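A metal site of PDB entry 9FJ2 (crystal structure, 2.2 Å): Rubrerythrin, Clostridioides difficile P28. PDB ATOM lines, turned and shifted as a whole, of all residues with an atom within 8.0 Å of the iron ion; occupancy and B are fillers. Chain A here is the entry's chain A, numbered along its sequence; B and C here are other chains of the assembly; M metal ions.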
ATOM      1  N   GLU A 144     -14.495  29.263 -24.845  1.00  0.00           N
ATOM      2  CA  GLU A 144     -13.097  29.001 -24.553  1.00  0.00           C
ATOM      3  C   GLU A 144     -12.730  29.645 -23.230  1.00  0.00           C
ATOM      4  O   GLU A 144     -13.070  30.802 -22.984  1.00  0.00           O
ATOM      5  CB  GLU A 144     -12.185  29.527 -25.670  1.00  0.00           C
ATOM      6  CG  GLU A 144     -10.709  29.579 -25.288  1.00  0.00           C
ATOM      7  CD  GLU A 144      -9.810  29.884 -26.471  1.00  0.00           C
ATOM      8  OE1 GLU A 144     -10.291  29.827 -27.616  1.00  0.00           O
ATOM      9  OE2 GLU A 144      -8.613  30.171 -26.246  1.00  0.00           O
ATOM     10  N   CYS A 145     -12.039  28.890 -22.370  1.00  0.00           N
ATOM     11  CA  CYS A 145     -11.542  29.411 -21.093  1.00  0.00           C
ATOM     12  C   CYS A 145     -10.256  30.182 -21.356  1.00  0.00           C
ATOM     13  O   CYS A 145      -9.242  29.604 -21.745  1.00  0.00           O
ATOM     14  CB  CYS A 145     -11.321  28.274 -20.110  1.00  0.00           C
ATOM     15  SG  CYS A 145     -10.650  28.772 -18.504  1.00  0.00           S
ATOM     16  N   LEU A 146     -10.286  31.500 -21.118  1.00  0.00           N
ATOM     17  CA  LEU A 146      -9.142  32.355 -21.408  1.00  0.00           C
ATOM     18  C   LEU A 146      -7.993  32.162 -20.437  1.00  0.00           C
ATOM     19  O   LEU A 146      -6.974  32.861 -20.561  1.00  0.00           O
ATOM     20  CB  LEU A 146      -9.586  33.821 -21.411  1.00  0.00           C
ATOM     21  CG  LEU A 146     -10.453  34.260 -22.588  1.00  0.00           C
ATOM     22  CD1 LEU A 146     -11.229  35.529 -22.248  1.00  0.00           C
ATOM     23  CD2 LEU A 146      -9.626  34.457 -23.845  1.00  0.00           C
ATOM     24  N   ASN A 147      -8.100  31.251 -19.471  1.00  0.00           N
ATOM     25  CA  ASN A 147      -7.028  30.986 -18.523  1.00  0.00           C
ATOM     26  C   ASN A 147      -6.255  29.711 -18.851  1.00  0.00           C
ATOM     27  O   ASN A 147      -5.034  29.725 -18.915  1.00  0.00           O
ATOM     28  CB  ASN A 147      -7.585  30.902 -17.104  1.00  0.00           C
ATOM     29  CG  ASN A 147      -6.505  30.676 -16.060  1.00  0.00           C
ATOM     30  OD1 ASN A 147      -6.313  29.569 -15.575  1.00  0.00           O
ATOM     31  ND2 ASN A 147      -5.785  31.741 -15.708  1.00  0.00           N
ATOM     32  N   CYS A 148      -6.969  28.594 -19.073  1.00  0.00           N
ATOM     33  CA  CYS A 148      -6.331  27.315 -19.327  1.00  0.00           C
ATOM     34  C   CYS A 148      -6.536  26.795 -20.743  1.00  0.00           C
ATOM     35  O   CYS A 148      -5.772  25.912 -21.172  1.00  0.00           O
ATOM     36  CB  CYS A 148      -6.845  26.259 -18.341  1.00  0.00           C
ATOM     37  SG  CYS A 148      -8.470  25.583 -18.757  1.00  0.00           S
ATOM     38  N   GLY A 149      -7.522  27.294 -21.471  1.00  0.00           N
ATOM     39  CA  GLY A 149      -7.799  26.833 -22.805  1.00  0.00           C
ATOM     40  C   GLY A 149      -8.862  25.764 -22.924  1.00  0.00           C
ATOM     41  O   GLY A 149      -8.942  25.115 -23.972  1.00  0.00           O
ATOM     42  N   HIS A 150      -9.679  25.566 -21.894  1.00  0.00           N
ATOM     43  CA  HIS A 150     -10.722  24.549 -21.947  1.00  0.00           C
ATOM     44  C   HIS A 150     -11.819  24.969 -22.916  1.00  0.00           C
ATOM     45  O   HIS A 150     -12.252  26.123 -22.937  1.00  0.00           O
ATOM     46  CB  HIS A 150     -11.315  24.336 -20.548  1.00  0.00           C
ATOM     47  CG  HIS A 150     -12.554  23.492 -20.544  1.00  0.00           C
ATOM     48  ND1 HIS A 150     -12.582  22.194 -20.997  1.00  0.00           N
ATOM     49  CD2 HIS A 150     -13.815  23.774 -20.132  1.00  0.00           C
ATOM     50  CE1 HIS A 150     -13.804  21.708 -20.869  1.00  0.00           C
ATOM     51  NE2 HIS A 150     -14.573  22.651 -20.343  1.00  0.00           N
ATOM     52  N   LEU A 151     -12.279  24.013 -23.715  1.00  0.00           N
ATOM     53  CA  LEU A 151     -13.356  24.228 -24.666  1.00  0.00           C
ATOM     54  C   LEU A 151     -14.636  23.594 -24.147  1.00  0.00           C
ATOM     55  O   LEU A 151     -14.633  22.460 -23.662  1.00  0.00           O
ATOM     56  CB  LEU A 151     -13.013  23.636 -26.040  1.00  0.00           C
ATOM     57  CG  LEU A 151     -12.098  24.490 -26.914  1.00  0.00           C
ATOM     58  CD1 LEU A 151     -11.942  23.877 -28.299  1.00  0.00           C
ATOM     59  CD2 LEU A 151     -12.648  25.904 -27.001  1.00  0.00           C
ATOM     60  N   VAL A 160     -18.224  27.375 -13.446  1.00  0.00           N
ATOM     61  CA  VAL A 160     -16.798  27.325 -13.130  1.00  0.00           C
ATOM     62  C   VAL A 160     -16.135  26.372 -14.103  1.00  0.00           C
ATOM     63  O   VAL A 160     -16.703  25.328 -14.450  1.00  0.00           O
ATOM     64  CB  VAL A 160     -16.546  26.885 -11.665  1.00  0.00           C
ATOM     65  CG1 VAL A 160     -15.068  26.684 -11.420  1.00  0.00           C
ATOM     66  CG2 VAL A 160     -17.121  27.901 -10.688  1.00  0.00           C
ATOM     67  N   CYS A 161     -14.947  26.746 -14.578  1.00  0.00           N
ATOM     68  CA  CYS A 161     -14.231  25.907 -15.527  1.00  0.00           C
ATOM     69  C   CYS A 161     -13.934  24.550 -14.899  1.00  0.00           C
ATOM     70  O   CYS A 161     -13.373  24.484 -13.794  1.00  0.00           O
ATOM     71  CB  CYS A 161     -12.929  26.578 -15.963  1.00  0.00           C
ATOM     72  SG  CYS A 161     -11.838  25.511 -16.918  1.00  0.00           S
ATOM     73  N   PRO A 162     -14.289  23.443 -15.560  1.00  0.00           N
ATOM     74  CA  PRO A 162     -14.071  22.113 -14.977  1.00  0.00           C
ATOM     75  C   PRO A 162     -12.659  21.571 -15.135  1.00  0.00           C
ATOM     76  O   PRO A 162     -12.427  20.401 -14.798  1.00  0.00           O
ATOM     77  CB  PRO A 162     -15.077  21.245 -15.744  1.00  0.00           C
ATOM     78  CG  PRO A 162     -15.193  21.895 -17.081  1.00  0.00           C
ATOM     79  CD  PRO A 162     -14.911  23.373 -16.892  1.00  0.00           C
ATOM     80  N   VAL A 163     -11.724  22.369 -15.625  1.00  0.00           N
ATOM     81  CA  VAL A 163     -10.326  21.955 -15.775  1.00  0.00           C
ATOM     82  C   VAL A 163      -9.420  22.690 -14.799  1.00  0.00           C
ATOM     83  O   VAL A 163      -8.737  22.068 -13.984  1.00  0.00           O
ATOM     84  CB  VAL A 163      -9.849  22.151 -17.241  1.00  0.00           C
ATOM     85  CG1 VAL A 163      -8.365  21.823 -17.358  1.00  0.00           C
ATOM     86  CG2 VAL A 163     -10.662  21.276 -18.182  1.00  0.00           C
ATOM     87  N   CYS A 164      -9.403  24.025 -14.852  1.00  0.00           N
ATOM     88  CA  CYS A 164      -8.544  24.840 -14.007  1.00  0.00           C
ATOM     89  C   CYS A 164      -9.289  25.482 -12.844  1.00  0.00           C
ATOM     90  O   CYS A 164      -8.663  26.141 -12.012  1.00  0.00           O
ATOM     91  CB  CYS A 164      -7.859  25.923 -14.834  1.00  0.00           C
ATOM     92  SG  CYS A 164      -8.990  27.139 -15.543  1.00  0.00           S
ATOM     93  N   ASN A 165     -10.623  25.320 -12.779  1.00  0.00           N
ATOM     94  CA  ASN A 165     -11.442  25.832 -11.677  1.00  0.00           C
ATOM     95  C   ASN A 165     -11.403  27.356 -11.623  1.00  0.00           C
ATOM     96  O   ASN A 165     -11.231  27.962 -10.561  1.00  0.00           O
ATOM     97  CB  ASN A 165     -11.018  25.217 -10.342  1.00  0.00           C
ATOM     98  CG  ASN A 165     -12.138  25.218  -9.314  1.00  0.00           C
ATOM     99  OD1 ASN A 165     -11.956  25.693  -8.190  1.00  0.00           O
ATOM    100  ND2 ASN A 165     -13.293  24.691  -9.692  1.00  0.00           N
ATOM    101  N   HIS A 166     -11.559  27.991 -12.781  1.00  0.00           N
ATOM    102  CA  HIS A 166     -11.676  29.439 -12.869  1.00  0.00           C
ATOM    103  C   HIS A 166     -13.114  29.843 -13.168  1.00  0.00           C
ATOM    104  O   HIS A 166     -13.851  29.092 -13.820  1.00  0.00           O
ATOM    105  CB  HIS A 166     -10.747  30.002 -13.955  1.00  0.00           C
ATOM    106  CG  HIS A 166      -9.355  30.284 -13.467  1.00  0.00           C
ATOM    107  ND1 HIS A 166      -8.512  29.294 -13.011  1.00  0.00           N
ATOM    108  CD2 HIS A 166      -8.660  31.432 -13.372  1.00  0.00           C
ATOM    109  CE1 HIS A 166      -7.359  29.820 -12.650  1.00  0.00           C
ATOM    110  NE2 HIS A 166      -7.423  31.128 -12.867  1.00  0.00           N
ATOM    111  N   PRO A 167     -13.570  31.016 -12.693  1.00  0.00           N
ATOM    112  CA  PRO A 167     -14.975  31.390 -12.878  1.00  0.00           C
ATOM    113  C   PRO A 167     -15.341  31.689 -14.330  1.00  0.00           C
ATOM    114  O   PRO A 167     -14.511  31.580 -15.227  1.00  0.00           O
ATOM    115  CB  PRO A 167     -15.112  32.648 -12.008  1.00  0.00           C
ATOM    116  CG  PRO A 167     -13.733  33.192 -11.890  1.00  0.00           C
ATOM    117  CD  PRO A 167     -12.822  32.000 -11.888  1.00  0.00           C
ATOM    118  N   TYR A 170     -13.526  34.225 -17.207  1.00  0.00           N
ATOM    119  CA  TYR A 170     -12.499  33.830 -18.158  1.00  0.00           C
ATOM    120  C   TYR A 170     -13.053  33.106 -19.385  1.00  0.00           C
ATOM    121  O   TYR A 170     -12.261  32.549 -20.156  1.00  0.00           O
ATOM    122  CB  TYR A 170     -11.462  32.933 -17.461  1.00  0.00           C
ATOM    123  CG  TYR A 170     -10.652  33.644 -16.397  1.00  0.00           C
ATOM    124  CD1 TYR A 170     -11.192  33.878 -15.138  1.00  0.00           C
ATOM    125  CD2 TYR A 170      -9.359  34.075 -16.654  1.00  0.00           C
ATOM    126  CE1 TYR A 170     -10.451  34.529 -14.162  1.00  0.00           C
ATOM    127  CE2 TYR A 170      -8.623  34.718 -15.683  1.00  0.00           C
ATOM    128  CZ  TYR A 170      -9.169  34.944 -14.446  1.00  0.00           C
ATOM    129  OH  TYR A 170      -8.440  35.588 -13.469  1.00  0.00           O
ATOM    130  N   PHE A 171     -14.363  33.096 -19.584  1.00  0.00           N
ATOM    131  CA  PHE A 171     -14.968  32.396 -20.720  1.00  0.00           C
ATOM    132  C   PHE A 171     -15.409  33.398 -21.776  1.00  0.00           C
ATOM    133  O   PHE A 171     -15.922  34.473 -21.465  1.00  0.00           O
ATOM    134  CB  PHE A 171     -16.162  31.555 -20.261  1.00  0.00           C
ATOM    135  CG  PHE A 171     -15.780  30.216 -19.720  1.00  0.00           C
ATOM    136  CD1 PHE A 171     -15.356  29.205 -20.581  1.00  0.00           C
ATOM    137  CD2 PHE A 171     -15.836  29.957 -18.365  1.00  0.00           C
ATOM    138  CE1 PHE A 171     -14.995  27.963 -20.082  1.00  0.00           C
ATOM    139  CE2 PHE A 171     -15.487  28.708 -17.864  1.00  0.00           C
ATOM    140  CZ  PHE A 171     -15.058  27.718 -18.721  1.00  0.00           C
ATOM    141  N   ILE B 114      -7.354  19.612 -24.305  1.00  0.00           N
ATOM    142  CA  ILE B 114      -6.873  20.925 -24.709  1.00  0.00           C
ATOM    143  C   ILE B 114      -5.673  20.793 -25.643  1.00  0.00           C
ATOM    144  O   ILE B 114      -5.563  21.504 -26.643  1.00  0.00           O
ATOM    145  CB  ILE B 114      -6.534  21.771 -23.472  1.00  0.00           C
ATOM    146  CG1 ILE B 114      -7.792  22.048 -22.653  1.00  0.00           C
ATOM    147  CG2 ILE B 114      -5.859  23.077 -23.870  1.00  0.00           C
ATOM    148  CD1 ILE B 114      -7.520  22.680 -21.301  1.00  0.00           C
ATOM    149  N   ASN C  51      -1.310  29.068 -21.658  1.00  0.00           N
ATOM    150  CA  ASN C  51      -2.170  27.920 -21.413  1.00  0.00           C
ATOM    151  C   ASN C  51      -1.398  26.789 -20.746  1.00  0.00           C
ATOM    152  O   ASN C  51      -1.863  26.192 -19.772  1.00  0.00           O
ATOM    153  CB  ASN C  51      -2.794  27.440 -22.729  1.00  0.00           C
ATOM    154  CG  ASN C  51      -4.025  28.222 -23.114  1.00  0.00           C
ATOM    155  OD1 ASN C  51      -4.570  28.984 -22.316  1.00  0.00           O
ATOM    156  ND2 ASN C  51      -4.480  28.042 -24.344  1.00  0.00           N
ATOM    157  N   GLU C  54      -0.690  27.440 -17.027  1.00  0.00           N
ATOM    158  CA  GLU C  54      -1.739  27.112 -16.070  1.00  0.00           C
ATOM    159  C   GLU C  54      -1.904  25.605 -15.905  1.00  0.00           C
ATOM    160  O   GLU C  54      -2.311  25.146 -14.827  1.00  0.00           O
ATOM    161  CB  GLU C  54      -3.059  27.738 -16.501  1.00  0.00           C
ATOM    162  CG  GLU C  54      -3.075  29.262 -16.435  1.00  0.00           C
ATOM    163  CD  GLU C  54      -2.965  29.790 -15.020  1.00  0.00           C
ATOM    164  OE1 GLU C  54      -3.570  29.176 -14.110  1.00  0.00           O
ATOM    165  OE2 GLU C  54      -2.288  30.821 -14.819  1.00  0.00           O
ATOM    166  N   HIS C  55      -1.619  24.821 -16.945  1.00  0.00           N
ATOM    167  CA  HIS C  55      -1.665  23.368 -16.814  1.00  0.00           C
ATOM    168  C   HIS C  55      -0.626  22.872 -15.819  1.00  0.00           C
ATOM    169  O   HIS C  55      -0.894  21.955 -15.031  1.00  0.00           O
ATOM    170  CB  HIS C  55      -1.456  22.700 -18.169  1.00  0.00           C
ATOM    171  CG  HIS C  55      -2.507  23.025 -19.186  1.00  0.00           C
ATOM    172  ND1 HIS C  55      -2.314  22.859 -20.535  1.00  0.00           N
ATOM    173  CD2 HIS C  55      -3.768  23.503 -19.037  1.00  0.00           C
ATOM    174  CE1 HIS C  55      -3.412  23.228 -21.186  1.00  0.00           C
ATOM    175  NE2 HIS C  55      -4.306  23.619 -20.298  1.00  0.00           N
ATOM    176  N   LEU C  58      -1.705  23.342 -12.177  1.00  0.00           N
ATOM    177  CA  LEU C  58      -2.588  22.304 -11.649  1.00  0.00           C
ATOM    178  C   LEU C  58      -1.778  21.164 -11.044  1.00  0.00           C
ATOM    179  O   LEU C  58      -2.035  20.727  -9.921  1.00  0.00           O
ATOM    180  CB  LEU C  58      -3.508  21.791 -12.754  1.00  0.00           C
ATOM    181  CG  LEU C  58      -4.539  22.786 -13.298  1.00  0.00           C
ATOM    182  CD1 LEU C  58      -5.372  22.138 -14.391  1.00  0.00           C
ATOM    183  CD2 LEU C  58      -5.426  23.306 -12.183  1.00  0.00           C
HETATM  184 FE    FE M   1     -10.039  26.767 -17.575  1.00  0.00          FE
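Of the 23 residues printed, 4 come within 4 Å of the iron ion. The nearest printed residue that does not touch the iron ion is His 150 (4.05 Å).
The iron ion is bound by the side-chain sulfur (SG) of Cys 161, the side-chain sulfur (SG) of Cys 145, the side-chain sulfur (SG) of Cys 148 and the side-chain sulfur (SG) of Cys 164.
The backbone carbonyl oxygen of Cys 164 lies within hydrogen-bond range of a ring nitrogen (ND1) of His 166. The backbone carbonyl oxygen (O) of Cys 148 is in hydrogen-bond range of a ring nitrogen (NE2) of His 55 of chain C (2.9 Å). N of Cys 161 sits at hydrogen-bond distance from O of His 166 (2.7 Å). The side-chain sulfur (SG) of Cys 145 lies close to the backbone NH (N) of Asn 147 (3.7 Å). The side-chain sulfur of Cys 148 sits close to the backbone NH of His 150 (3.4 Å). O of His 150 sits at hydrogen-bond distance from N of Cys 145 (2.8 Å). OD1 of Asn 51 of chain C sits close to O of Cys 148, 3.5 Å away. The side-chain sulfur (SG) of Cys 164 lies close to the side-chain amide oxygen (OD1) of Asn 147 (3.6 Å).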
